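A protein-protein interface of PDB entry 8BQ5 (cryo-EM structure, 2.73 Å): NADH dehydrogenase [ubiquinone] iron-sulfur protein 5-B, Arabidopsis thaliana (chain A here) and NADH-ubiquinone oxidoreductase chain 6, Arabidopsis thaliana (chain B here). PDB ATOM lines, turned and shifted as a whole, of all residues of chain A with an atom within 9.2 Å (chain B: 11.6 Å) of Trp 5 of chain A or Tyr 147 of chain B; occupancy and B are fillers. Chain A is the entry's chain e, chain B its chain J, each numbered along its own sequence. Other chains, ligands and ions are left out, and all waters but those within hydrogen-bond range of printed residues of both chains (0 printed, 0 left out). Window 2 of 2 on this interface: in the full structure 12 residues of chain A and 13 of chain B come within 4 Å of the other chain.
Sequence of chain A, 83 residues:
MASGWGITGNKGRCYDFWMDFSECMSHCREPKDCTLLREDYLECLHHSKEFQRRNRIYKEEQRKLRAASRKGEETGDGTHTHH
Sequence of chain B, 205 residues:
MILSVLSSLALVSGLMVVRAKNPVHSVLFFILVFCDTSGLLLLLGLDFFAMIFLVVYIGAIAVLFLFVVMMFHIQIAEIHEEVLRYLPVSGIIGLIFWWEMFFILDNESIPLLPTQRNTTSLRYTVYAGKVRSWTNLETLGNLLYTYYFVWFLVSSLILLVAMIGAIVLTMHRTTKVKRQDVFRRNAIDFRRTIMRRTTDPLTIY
O of Thr 135 of chain B lies within hydrogen-bond range of OG1 of Thr 139 of chain B (2.9 Å).
O of Asn 142 of chain B sits at hydrogen-bond distance from OG1 of Thr 146 of chain B (3.2 Å).
O of Leu 143 of chain B is in hydrogen-bond range of N of Tyr 148 of chain B (3.4 Å).
The side-chain hydroxyl (OG) of Ser 3 of chain A lies close to the backbone NH (N) of Trp 5 of chain A (3.4 Å).
Among the printed residues, pairs that only touch across the chains: Trp 5 of chain A with Leu 143 of chain B (3.4 Å), Gly 6 of chain A with Thr 139 of chain B (3.4 Å), Gly 9 of chain A with Trp 134 of chain B (3.5 Å), Ile 7 of chain A with Thr 139 of chain B (3.8 Å), Thr 8 of chain A with Trp 134 of chain B (3.8 Å), Trp 5 of chain A with Tyr 147 of chain B (3.9 Å), Trp 5 of chain A with Asn 142 of chain B (3.9 Å) and Trp 5 of chain A with Tyr 148 of chain B (3.9 Å).
Ser 3 of chain A touches none of the printed residues of chain B.
Of chain B, only Asn 142 (3.9 Å), Leu 143 (3.4 Å), Tyr 147 (3.9 Å) and Tyr 148 (3.9 Å) come within 4 Å of Trp 5 of chain A.
Of chain B, only Thr 139 (3.4 Å) comes within 4 Å of Gly 6 of chain A.
Of the printed residues of chain B, Ile 7 of chain A touches Thr 139.
No residue of chain B comes within 4 Å of Gly 12 of chain A.
Of the printed residues of chain A, Trp 134 of chain B touches Thr 8 (3.8 Å) and Gly 9 (3.5 Å).
Printed residues of chain A within 4 Å of Thr 139 of chain B: Gly 6 and Ile 7.
Printed residues of chain A within 4 Å of Asn 142 of chain B: Trp 5.
Printed residues of chain A within 4 Å of Leu 143 of chain B: Trp 5 (3.4 Å).
Thr 146 of chain B touches none of the printed residues of chain A.
Tyr 147 of chain B touches just one residue of chain A: Trp 5.
Of the printed residues of chain A, Tyr 148 of chain B touches Trp 5.
The nearest residue of chain B that does not touch Trp 5 of chain A is Thr 139 of chain B (6.2 Å).
Printed residues of chain B that touch a printed residue of chain A: Trp 134, Thr 139, Asn 142, Leu 143, Tyr 147 and Tyr 148.
Hydrophobic or aromatic side chains of chain B that line the printed part of chain A: Trp 134, Leu 143, Tyr 147 and Tyr 148.
Along chain B the printed residues that touch a printed residue of chain A span positions 134 to 148.
Of the 14 printed residues of chain A, 5 touch a printed residue of chain B.
Hydrophobic or aromatic side chains of chain A that line the printed part of chain B: Trp 5.
Among the printed residues, no Asp or Glu carboxylate lies within 4 Å of a Lys or Arg side-chain nitrogen of the other chain.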
ATOM      1  N   ALA A   2      31.683 -17.869 -20.453  1.00  0.00           N
ATOM      2  CA  ALA A   2      30.472 -17.374 -21.098  1.00  0.00           C
ATOM      3  C   ALA A   2      29.434 -16.891 -20.086  1.00  0.00           C
ATOM      4  O   ALA A   2      28.539 -16.125 -20.432  1.00  0.00           O
ATOM      5  CB  ALA A   2      29.872 -18.452 -21.989  1.00  0.00           C
ATOM      6  N   SER A   3      29.548 -17.344 -18.834  1.00  0.00           N
ATOM      7  CA  SER A   3      28.546 -16.983 -17.835  1.00  0.00           C
ATOM      8  C   SER A   3      28.826 -15.620 -17.214  1.00  0.00           C
ATOM      9  O   SER A   3      27.896 -14.947 -16.757  1.00  0.00           O
ATOM     10  CB  SER A   3      28.469 -18.058 -16.749  1.00  0.00           C
ATOM     11  OG  SER A   3      29.474 -17.876 -15.768  1.00  0.00           O
ATOM     12  N   GLY A   4      30.089 -15.201 -17.180  1.00  0.00           N
ATOM     13  CA  GLY A   4      30.453 -13.909 -16.648  1.00  0.00           C
ATOM     14  C   GLY A   4      30.760 -13.872 -15.168  1.00  0.00           C
ATOM     15  O   GLY A   4      31.227 -12.838 -14.678  1.00  0.00           O
ATOM     16  N   TRP A   5      30.516 -14.959 -14.438  1.00  0.00           N
ATOM     17  CA  TRP A   5      30.843 -15.015 -13.016  1.00  0.00           C
ATOM     18  C   TRP A   5      32.299 -15.435 -12.862  1.00  0.00           C
ATOM     19  O   TRP A   5      32.652 -16.584 -13.143  1.00  0.00           O
ATOM     20  CB  TRP A   5      29.923 -15.987 -12.284  1.00  0.00           C
ATOM     21  CG  TRP A   5      28.457 -15.709 -12.425  1.00  0.00           C
ATOM     22  CD1 TRP A   5      27.570 -16.374 -13.218  1.00  0.00           C
ATOM     23  CD2 TRP A   5      27.703 -14.709 -11.733  1.00  0.00           C
ATOM     24  NE1 TRP A   5      26.312 -15.847 -13.069  1.00  0.00           N
ATOM     25  CE2 TRP A   5      26.365 -14.823 -12.161  1.00  0.00           C
ATOM     26  CE3 TRP A   5      28.027 -13.727 -10.791  1.00  0.00           C
ATOM     27  CZ2 TRP A   5      25.356 -13.992 -11.686  1.00  0.00           C
ATOM     28  CZ3 TRP A   5      27.023 -12.903 -10.319  1.00  0.00           C
ATOM     29  CH2 TRP A   5      25.704 -13.041 -10.766  1.00  0.00           C
ATOM     30  N   GLY A   6      33.146 -14.512 -12.413  1.00  0.00           N
ATOM     31  CA  GLY A   6      34.539 -14.837 -12.206  1.00  0.00           C
ATOM     32  C   GLY A   6      34.784 -15.544 -10.888  1.00  0.00           C
ATOM     33  O   GLY A   6      34.031 -15.410  -9.925  1.00  0.00           O
ATOM     34  N   ILE A   7      35.880 -16.304 -10.842  1.00  0.00           N
ATOM     35  CA  ILE A   7      36.190 -17.093  -9.655  1.00  0.00           C
ATOM     36  C   ILE A   7      36.719 -16.254  -8.503  1.00  0.00           C
ATOM     37  O   ILE A   7      36.998 -16.800  -7.431  1.00  0.00           O
ATOM     38  CB  ILE A   7      37.184 -18.218 -10.006  1.00  0.00           C
ATOM     39  CG1 ILE A   7      38.516 -17.640 -10.480  1.00  0.00           C
ATOM     40  CG2 ILE A   7      36.590 -19.141 -11.056  1.00  0.00           C
ATOM     41  CD1 ILE A   7      39.574 -18.688 -10.720  1.00  0.00           C
ATOM     42  N   THR A   8      36.852 -14.940  -8.686  1.00  0.00           N
ATOM     43  CA  THR A   8      37.254 -14.043  -7.610  1.00  0.00           C
ATOM     44  C   THR A   8      36.238 -12.937  -7.356  1.00  0.00           C
ATOM     45  O   THR A   8      36.579 -11.932  -6.724  1.00  0.00           O
ATOM     46  CB  THR A   8      38.624 -13.425  -7.901  1.00  0.00           C
ATOM     47  OG1 THR A   8      38.548 -12.623  -9.086  1.00  0.00           O
ATOM     48  CG2 THR A   8      39.675 -14.509  -8.085  1.00  0.00           C
ATOM     49  N   GLY A   9      35.007 -13.085  -7.833  1.00  0.00           N
ATOM     50  CA  GLY A   9      33.973 -12.110  -7.562  1.00  0.00           C
ATOM     51  C   GLY A   9      33.926 -10.917  -8.488  1.00  0.00           C
ATOM     52  O   GLY A   9      33.315  -9.904  -8.131  1.00  0.00           O
ATOM     53  N   ASN A  10      34.557 -10.993  -9.657  1.00  0.00           N
ATOM     54  CA  ASN A  10      34.490  -9.947 -10.670  1.00  0.00           C
ATOM     55  C   ASN A  10      34.061 -10.563 -11.994  1.00  0.00           C
ATOM     56  O   ASN A  10      33.861 -11.776 -12.100  1.00  0.00           O
ATOM     57  CB  ASN A  10      35.831  -9.219 -10.822  1.00  0.00           C
ATOM     58  CG  ASN A  10      36.029  -8.142  -9.782  1.00  0.00           C
ATOM     59  OD1 ASN A  10      35.322  -7.134  -9.774  1.00  0.00           O
ATOM     60  ND2 ASN A  10      36.998  -8.342  -8.901  1.00  0.00           N
ATOM     61  N   LYS A  11      33.918  -9.717 -13.010  1.00  0.00           N
ATOM     62  CA  LYS A  11      33.557 -10.202 -14.335  1.00  0.00           C
ATOM     63  C   LYS A  11      34.616 -11.173 -14.841  1.00  0.00           C
ATOM     64  O   LYS A  11      35.816 -10.934 -14.686  1.00  0.00           O
ATOM     65  CB  LYS A  11      33.404  -9.032 -15.311  1.00  0.00           C
ATOM     66  CG  LYS A  11      33.365  -9.462 -16.771  1.00  0.00           C
ATOM     67  CD  LYS A  11      33.141  -8.303 -17.730  1.00  0.00           C
ATOM     68  CE  LYS A  11      32.164  -7.289 -17.176  1.00  0.00           C
ATOM     69  NZ  LYS A  11      32.389  -5.947 -17.774  1.00  0.00           N
ATOM     70  N   GLY A  12      34.166 -12.270 -15.445  1.00  0.00           N
ATOM     71  CA  GLY A  12      35.071 -13.268 -15.978  1.00  0.00           C
ATOM     72  C   GLY A  12      36.020 -12.711 -17.019  1.00  0.00           C
ATOM     73  O   GLY A  12      35.714 -11.714 -17.679  1.00  0.00           O
ATOM     74  N   ARG A  13      37.182 -13.355 -17.172  1.00  0.00           N
ATOM     75  CA  ARG A  13      38.224 -12.822 -18.046  1.00  0.00           C
ATOM     76  C   ARG A  13      37.763 -12.758 -19.496  1.00  0.00           C
ATOM     77  O   ARG A  13      38.033 -11.779 -20.200  1.00  0.00           O
ATOM     78  CB  ARG A  13      39.490 -13.670 -17.923  1.00  0.00           C
ATOM     79  CG  ARG A  13      40.483 -13.486 -19.062  1.00  0.00           C
ATOM     80  CD  ARG A  13      41.724 -14.337 -18.857  1.00  0.00           C
ATOM     81  NE  ARG A  13      41.672 -15.583 -19.614  1.00  0.00           N
ATOM     82  CZ  ARG A  13      41.502 -16.778 -19.069  1.00  0.00           C
ATOM     83  NH1 ARG A  13      41.349 -16.925 -17.764  1.00  0.00           N
ATOM     84  NH2 ARG A  13      41.482 -17.853 -19.852  1.00  0.00           N
ATOM     85  N   CYS A  14      37.058 -13.787 -19.959  1.00  0.00           N
ATOM     86  CA  CYS A  14      36.695 -13.924 -21.361  1.00  0.00           C
ATOM     87  C   CYS A  14      35.247 -13.550 -21.641  1.00  0.00           C
ATOM     88  O   CYS A  14      34.733 -13.874 -22.715  1.00  0.00           O
ATOM     89  CB  CYS A  14      36.966 -15.354 -21.823  1.00  0.00           C
ATOM     90  SG  CYS A  14      38.690 -15.833 -21.660  1.00  0.00           S
ATOM     91  N   TYR A  15      34.581 -12.872 -20.706  1.00  0.00           N
ATOM     92  CA  TYR A  15      33.151 -12.628 -20.854  1.00  0.00           C
ATOM     93  C   TYR A  15      32.861 -11.598 -21.938  1.00  0.00           C
ATOM     94  O   TYR A  15      31.886 -11.737 -22.681  1.00  0.00           O
ATOM     95  CB  TYR A  15      32.554 -12.181 -19.523  1.00  0.00           C
ATOM     96  CG  TYR A  15      31.082 -11.862 -19.601  1.00  0.00           C
ATOM     97  CD1 TYR A  15      30.153 -12.856 -19.881  1.00  0.00           C
ATOM     98  CD2 TYR A  15      30.622 -10.569 -19.406  1.00  0.00           C
ATOM     99  CE1 TYR A  15      28.807 -12.572 -19.949  1.00  0.00           C
ATOM    100  CE2 TYR A  15      29.279 -10.275 -19.475  1.00  0.00           C
ATOM    101  CZ  TYR A  15      28.375 -11.281 -19.746  1.00  0.00           C
ATOM    102  OH  TYR A  15      27.034 -10.992 -19.818  1.00  0.00           O
ATOM    103  N   LEU B  46      41.613 -23.445  -4.376  1.00  0.00           N
ATOM    104  CA  LEU B  46      40.224 -23.685  -3.984  1.00  0.00           C
ATOM    105  C   LEU B  46      40.226 -24.403  -2.637  1.00  0.00           C
ATOM    106  O   LEU B  46      40.129 -25.627  -2.549  1.00  0.00           O
ATOM    107  CB  LEU B  46      39.503 -24.491  -5.060  1.00  0.00           C
ATOM    108  CG  LEU B  46      39.747 -24.039  -6.500  1.00  0.00           C
ATOM    109  CD1 LEU B  46      39.333 -25.119  -7.482  1.00  0.00           C
ATOM    110  CD2 LEU B  46      39.006 -22.743  -6.783  1.00  0.00           C
ATOM    111  N   TRP B 134      37.354 -11.675  -2.530  1.00  0.00           N
ATOM    112  CA  TRP B 134      36.364 -12.684  -2.183  1.00  0.00           C
ATOM    113  C   TRP B 134      37.057 -14.026  -1.999  1.00  0.00           C
ATOM    114  O   TRP B 134      37.921 -14.401  -2.796  1.00  0.00           O
ATOM    115  CB  TRP B 134      35.299 -12.813  -3.274  1.00  0.00           C
ATOM    116  CG  TRP B 134      34.200 -11.796  -3.220  1.00  0.00           C
ATOM    117  CD1 TRP B 134      34.240 -10.574  -2.618  1.00  0.00           C
ATOM    118  CD2 TRP B 134      32.902 -11.905  -3.820  1.00  0.00           C
ATOM    119  NE1 TRP B 134      33.045  -9.920  -2.795  1.00  0.00           N
ATOM    120  CE2 TRP B 134      32.206 -10.716  -3.530  1.00  0.00           C
ATOM    121  CE3 TRP B 134      32.258 -12.897  -4.568  1.00  0.00           C
ATOM    122  CZ2 TRP B 134      30.902 -10.490  -3.963  1.00  0.00           C
ATOM    123  CZ3 TRP B 134      30.963 -12.669  -4.997  1.00  0.00           C
ATOM    124  CH2 TRP B 134      30.300 -11.477  -4.693  1.00  0.00           C
ATOM    125  N   THR B 135      36.678 -14.750  -0.952  1.00  0.00           N
ATOM    126  CA  THR B 135      37.144 -16.120  -0.838  1.00  0.00           C
ATOM    127  C   THR B 135      36.361 -17.012  -1.797  1.00  0.00           C
ATOM    128  O   THR B 135      35.308 -16.638  -2.318  1.00  0.00           O
ATOM    129  CB  THR B 135      37.008 -16.630   0.598  1.00  0.00           C
ATOM    130  OG1 THR B 135      35.633 -16.901   0.890  1.00  0.00           O
ATOM    131  CG2 THR B 135      37.538 -15.602   1.582  1.00  0.00           C
ATOM    132  N   ASN B 136      36.905 -18.204  -2.046  1.00  0.00           N
ATOM    133  CA  ASN B 136      36.207 -19.169  -2.887  1.00  0.00           C
ATOM    134  C   ASN B 136      34.858 -19.530  -2.269  1.00  0.00           C
ATOM    135  O   ASN B 136      33.865 -19.748  -2.982  1.00  0.00           O
ATOM    136  CB  ASN B 136      37.112 -20.393  -3.091  1.00  0.00           C
ATOM    137  CG  ASN B 136      36.360 -21.634  -3.520  1.00  0.00           C
ATOM    138  OD1 ASN B 136      35.540 -21.596  -4.432  1.00  0.00           O
ATOM    139  ND2 ASN B 136      36.684 -22.758  -2.898  1.00  0.00           N
ATOM    140  N   GLU B 138      32.875 -17.415  -0.427  1.00  0.00           N
ATOM    141  CA  GLU B 138      31.909 -16.360  -0.722  1.00  0.00           C
ATOM    142  C   GLU B 138      31.506 -16.342  -2.188  1.00  0.00           C
ATOM    143  O   GLU B 138      30.345 -16.062  -2.497  1.00  0.00           O
ATOM    144  CB  GLU B 138      32.436 -14.976  -0.346  1.00  0.00           C
ATOM    145  CG  GLU B 138      33.255 -14.877   0.913  1.00  0.00           C
ATOM    146  CD  GLU B 138      33.971 -13.544   0.997  1.00  0.00           C
ATOM    147  OE1 GLU B 138      35.103 -13.496   1.518  1.00  0.00           O
ATOM    148  OE2 GLU B 138      33.397 -12.540   0.526  1.00  0.00           O
ATOM    149  N   THR B 139      32.439 -16.613  -3.100  1.00  0.00           N
ATOM    150  CA  THR B 139      32.079 -16.630  -4.512  1.00  0.00           C
ATOM    151  C   THR B 139      31.067 -17.732  -4.806  1.00  0.00           C
ATOM    152  O   THR B 139      30.108 -17.516  -5.555  1.00  0.00           O
ATOM    153  CB  THR B 139      33.329 -16.782  -5.379  1.00  0.00           C
ATOM    154  OG1 THR B 139      34.334 -15.866  -4.933  1.00  0.00           O
ATOM    155  CG2 THR B 139      33.001 -16.464  -6.823  1.00  0.00           C
ATOM    156  N   LEU B 140      31.249 -18.919  -4.212  1.00  0.00           N
ATOM    157  CA  LEU B 140      30.263 -19.984  -4.402  1.00  0.00           C
ATOM    158  C   LEU B 140      28.924 -19.641  -3.750  1.00  0.00           C
ATOM    159  O   LEU B 140      27.854 -19.869  -4.341  1.00  0.00           O
ATOM    160  CB  LEU B 140      30.806 -21.300  -3.844  1.00  0.00           C
ATOM    161  CG  LEU B 140      30.146 -22.586  -4.342  1.00  0.00           C
ATOM    162  CD1 LEU B 140      29.861 -22.505  -5.832  1.00  0.00           C
ATOM    163  CD2 LEU B 140      31.029 -23.780  -4.028  1.00  0.00           C
ATOM    164  N   GLY B 141      28.963 -19.095  -2.530  1.00  0.00           N
ATOM    165  CA  GLY B 141      27.744 -18.774  -1.812  1.00  0.00           C
ATOM    166  C   GLY B 141      26.967 -17.624  -2.409  1.00  0.00           C
ATOM    167  O   GLY B 141      25.767 -17.496  -2.142  1.00  0.00           O
ATOM    168  N   ASN B 142      27.625 -16.777  -3.199  1.00  0.00           N
ATOM    169  CA  ASN B 142      26.919 -15.726  -3.917  1.00  0.00           C
ATOM    170  C   ASN B 142      25.985 -16.284  -4.984  1.00  0.00           C
ATOM    171  O   ASN B 142      25.016 -15.614  -5.355  1.00  0.00           O
ATOM    172  CB  ASN B 142      27.931 -14.776  -4.559  1.00  0.00           C
ATOM    173  CG  ASN B 142      27.270 -13.649  -5.315  1.00  0.00           C
ATOM    174  OD1 ASN B 142      26.340 -13.016  -4.818  1.00  0.00           O
ATOM    175  ND2 ASN B 142      27.734 -13.402  -6.532  1.00  0.00           N
ATOM    176  N   LEU B 143      26.247 -17.494  -5.475  1.00  0.00           N
ATOM    177  CA  LEU B 143      25.522 -18.058  -6.606  1.00  0.00           C
ATOM    178  C   LEU B 143      24.599 -19.209  -6.252  1.00  0.00           C
ATOM    179  O   LEU B 143      23.564 -19.364  -6.903  1.00  0.00           O
ATOM    180  CB  LEU B 143      26.502 -18.555  -7.672  1.00  0.00           C
ATOM    181  CG  LEU B 143      27.472 -17.533  -8.246  1.00  0.00           C
ATOM    182  CD1 LEU B 143      28.456 -18.226  -9.163  1.00  0.00           C
ATOM    183  CD2 LEU B 143      26.695 -16.471  -8.985  1.00  0.00           C
ATOM    184  N   LEU B 144      24.954 -20.025  -5.255  1.00  0.00           N
ATOM    185  CA  LEU B 144      24.229 -21.277  -5.041  1.00  0.00           C
ATOM    186  C   LEU B 144      22.744 -21.053  -4.778  1.00  0.00           C
ATOM    187  O   LEU B 144      21.893 -21.762  -5.330  1.00  0.00           O
ATOM    188  CB  LEU B 144      24.847 -22.046  -3.876  1.00  0.00           C
ATOM    189  CG  LEU B 144      26.087 -22.867  -4.200  1.00  0.00           C
ATOM    190  CD1 LEU B 144      26.615 -23.499  -2.929  1.00  0.00           C
ATOM    191  CD2 LEU B 144      25.768 -23.918  -5.254  1.00  0.00           C
ATOM    192  N   TYR B 145      22.411 -20.084  -3.935  1.00  0.00           N
ATOM    193  CA  TYR B 145      21.076 -19.995  -3.364  1.00  0.00           C
ATOM    194  C   TYR B 145      20.176 -18.984  -4.059  1.00  0.00           C
ATOM    195  O   TYR B 145      18.994 -18.896  -3.710  1.00  0.00           O
ATOM    196  CB  TYR B 145      21.190 -19.663  -1.872  1.00  0.00           C
ATOM    197  CG  TYR B 145      22.298 -20.452  -1.219  1.00  0.00           C
ATOM    198  CD1 TYR B 145      22.096 -21.766  -0.820  1.00  0.00           C
ATOM    199  CD2 TYR B 145      23.560 -19.902  -1.049  1.00  0.00           C
ATOM    200  CE1 TYR B 145      23.111 -22.498  -0.244  1.00  0.00           C
ATOM    201  CE2 TYR B 145      24.580 -20.628  -0.478  1.00  0.00           C
ATOM    202  CZ  TYR B 145      24.352 -21.923  -0.076  1.00  0.00           C
ATOM    203  OH  TYR B 145      25.370 -22.645   0.496  1.00  0.00           O
ATOM    204  N   THR B 146      20.695 -18.206  -5.009  1.00  0.00           N
ATOM    205  CA  THR B 146      19.873 -17.217  -5.697  1.00  0.00           C
ATOM    206  C   THR B 146      19.769 -17.460  -7.198  1.00  0.00           C
ATOM    207  O   THR B 146      18.667 -17.705  -7.698  1.00  0.00           O
ATOM    208  CB  THR B 146      20.435 -15.821  -5.416  1.00  0.00           C
ATOM    209  OG1 THR B 146      21.842 -15.818  -5.678  1.00  0.00           O
ATOM    210  CG2 THR B 146      20.200 -15.445  -3.964  1.00  0.00           C
ATOM    211  N   TYR B 147      20.886 -17.445  -7.928  1.00  0.00           N
ATOM    212  CA  TYR B 147      20.823 -17.501  -9.383  1.00  0.00           C
ATOM    213  C   TYR B 147      20.737 -18.921  -9.919  1.00  0.00           C
ATOM    214  O   TYR B 147      20.344 -19.108 -11.075  1.00  0.00           O
ATOM    215  CB  TYR B 147      22.029 -16.778  -9.993  1.00  0.00           C
ATOM    216  CG  TYR B 147      22.057 -15.311  -9.647  1.00  0.00           C
ATOM    217  CD1 TYR B 147      21.315 -14.398 -10.379  1.00  0.00           C
ATOM    218  CD2 TYR B 147      22.804 -14.838  -8.577  1.00  0.00           C
ATOM    219  CE1 TYR B 147      21.318 -13.061 -10.066  1.00  0.00           C
ATOM    220  CE2 TYR B 147      22.815 -13.496  -8.255  1.00  0.00           C
ATOM    221  CZ  TYR B 147      22.069 -12.613  -9.007  1.00  0.00           C
ATOM    222  OH  TYR B 147      22.062 -11.274  -8.703  1.00  0.00           O
ATOM    223  N   TYR B 148      21.070 -19.918  -9.111  1.00  0.00           N
ATOM    224  CA  TYR B 148      20.989 -21.315  -9.514  1.00  0.00           C
ATOM    225  C   TYR B 148      20.350 -22.152  -8.416  1.00  0.00           C
ATOM    226  O   TYR B 148      20.778 -23.274  -8.134  1.00  0.00           O
ATOM    227  CB  TYR B 148      22.370 -21.846  -9.893  1.00  0.00           C
ATOM    228  CG  TYR B 148      22.969 -21.129 -11.083  1.00  0.00           C
ATOM    229  CD1 TYR B 148      22.625 -21.492 -12.378  1.00  0.00           C
ATOM    230  CD2 TYR B 148      23.852 -20.072 -10.913  1.00  0.00           C
ATOM    231  CE1 TYR B 148      23.158 -20.839 -13.470  1.00  0.00           C
ATOM    232  CE2 TYR B 148      24.389 -19.410 -12.000  1.00  0.00           C
ATOM    233  CZ  TYR B 148      24.038 -19.798 -13.277  1.00  0.00           C
ATOM    234  OH  TYR B 148      24.567 -19.145 -14.363  1.00  0.00           O
ATOM    235  N   PHE B 149      19.294 -21.621  -7.793  1.00  0.00           N
ATOM    236  CA  PHE B 149      18.702 -22.278  -6.631  1.00  0.00           C
ATOM    237  C   PHE B 149      17.888 -23.515  -7.010  1.00  0.00           C
ATOM    238  O   PHE B 149      17.703 -24.410  -6.175  1.00  0.00           O
ATOM    239  CB  PHE B 149      17.844 -21.279  -5.847  1.00  0.00           C
ATOM    240  CG  PHE B 149      16.503 -20.992  -6.467  1.00  0.00           C
ATOM    241  CD1 PHE B 149      16.362 -19.999  -7.419  1.00  0.00           C
ATOM    242  CD2 PHE B 149      15.375 -21.692  -6.072  1.00  0.00           C
ATOM    243  CE1 PHE B 149      15.133 -19.732  -7.989  1.00  0.00           C
ATOM    244  CE2 PHE B 149      14.145 -21.425  -6.634  1.00  0.00           C
ATOM    245  CZ  PHE B 149      14.024 -20.442  -7.592  1.00  0.00           C
ATOM    246  N   VAL B 150      17.393 -23.586  -8.249  1.00  0.00           N
ATOM    247  CA  VAL B 150      16.608 -24.749  -8.662  1.00  0.00           C
ATOM    248  C   VAL B 150      17.461 -26.013  -8.632  1.00  0.00           C
ATOM    249  O   VAL B 150      17.007 -27.076  -8.189  1.00  0.00           O
ATOM    250  CB  VAL B 150      15.985 -24.514 -10.051  1.00  0.00           C
ATOM    251  CG1 VAL B 150      15.214 -25.743 -10.496  1.00  0.00           C
ATOM    252  CG2 VAL B 150      15.065 -23.306 -10.015  1.00  0.00           C
ATOM    253  N   TRP B 151      18.706 -25.922  -9.106  1.00  0.00           N
ATOM    254  CA  TRP B 151      19.605 -27.074  -9.064  1.00  0.00           C
ATOM    255  C   TRP B 151      19.915 -27.481  -7.625  1.00  0.00           C
ATOM    256  O   TRP B 151      20.010 -28.675  -7.310  1.00  0.00           O
ATOM    257  CB  TRP B 151      20.887 -26.757  -9.836  1.00  0.00           C
ATOM    258  CG  TRP B 151      20.657 -26.292 -11.257  1.00  0.00           C
ATOM    259  CD1 TRP B 151      19.515 -26.431 -11.993  1.00  0.00           C
ATOM    260  CD2 TRP B 151      21.608 -25.648 -12.116  1.00  0.00           C
ATOM    261  NE1 TRP B 151      19.690 -25.901 -13.246  1.00  0.00           N
ATOM    262  CE2 TRP B 151      20.966 -25.415 -13.348  1.00  0.00           C
ATOM    263  CE3 TRP B 151      22.934 -25.236 -11.958  1.00  0.00           C
ATOM    264  CZ2 TRP B 151      21.607 -24.794 -14.416  1.00  0.00           C
ATOM    265  CZ3 TRP B 151      23.569 -24.625 -13.021  1.00  0.00           C
ATOM    266  CH2 TRP B 151      22.905 -24.405 -14.233  1.00  0.00           C
ATOM    267  N   PHE B 152      20.066 -26.494  -6.741  1.00  0.00           N
ATOM    268  CA  PHE B 152      20.234 -26.728  -5.310  1.00  0.00           C
ATOM    269  C   PHE B 152      19.076 -27.552  -4.741  1.00  0.00           C
ATOM    270  O   PHE B 152      19.278 -28.572  -4.059  1.00  0.00           O
ATOM    271  CB  PHE B 152      20.350 -25.351  -4.641  1.00  0.00           C
ATOM    272  CG  PHE B 152      20.471 -25.369  -3.149  1.00  0.00           C
ATOM    273  CD1 PHE B 152      21.442 -26.120  -2.515  1.00  0.00           C
ATOM    274  CD2 PHE B 152      19.645 -24.562  -2.381  1.00  0.00           C
ATOM    275  CE1 PHE B 152      21.555 -26.099  -1.138  1.00  0.00           C
ATOM    276  CE2 PHE B 152      19.755 -24.539  -1.011  1.00  0.00           C
ATOM    277  CZ  PHE B 152      20.712 -25.306  -0.388  1.00  0.00           C
ATOM    278  N   LEU B 153      17.845 -27.145  -5.054  1.00  0.00           N
ATOM    279  CA  LEU B 153      16.682 -27.858  -4.534  1.00  0.00           C
ATOM    280  C   LEU B 153      16.552 -29.252  -5.149  1.00  0.00           C
ATOM    281  O   LEU B 153      16.123 -30.199  -4.475  1.00  0.00           O
ATOM    282  CB  LEU B 153      15.424 -27.026  -4.770  1.00  0.00           C
ATOM    283  CG  LEU B 153      15.430 -25.682  -4.039  1.00  0.00           C
ATOM    284  CD1 LEU B 153      14.121 -24.944  -4.243  1.00  0.00           C
ATOM    285  CD2 LEU B 153      15.713 -25.878  -2.557  1.00  0.00           C
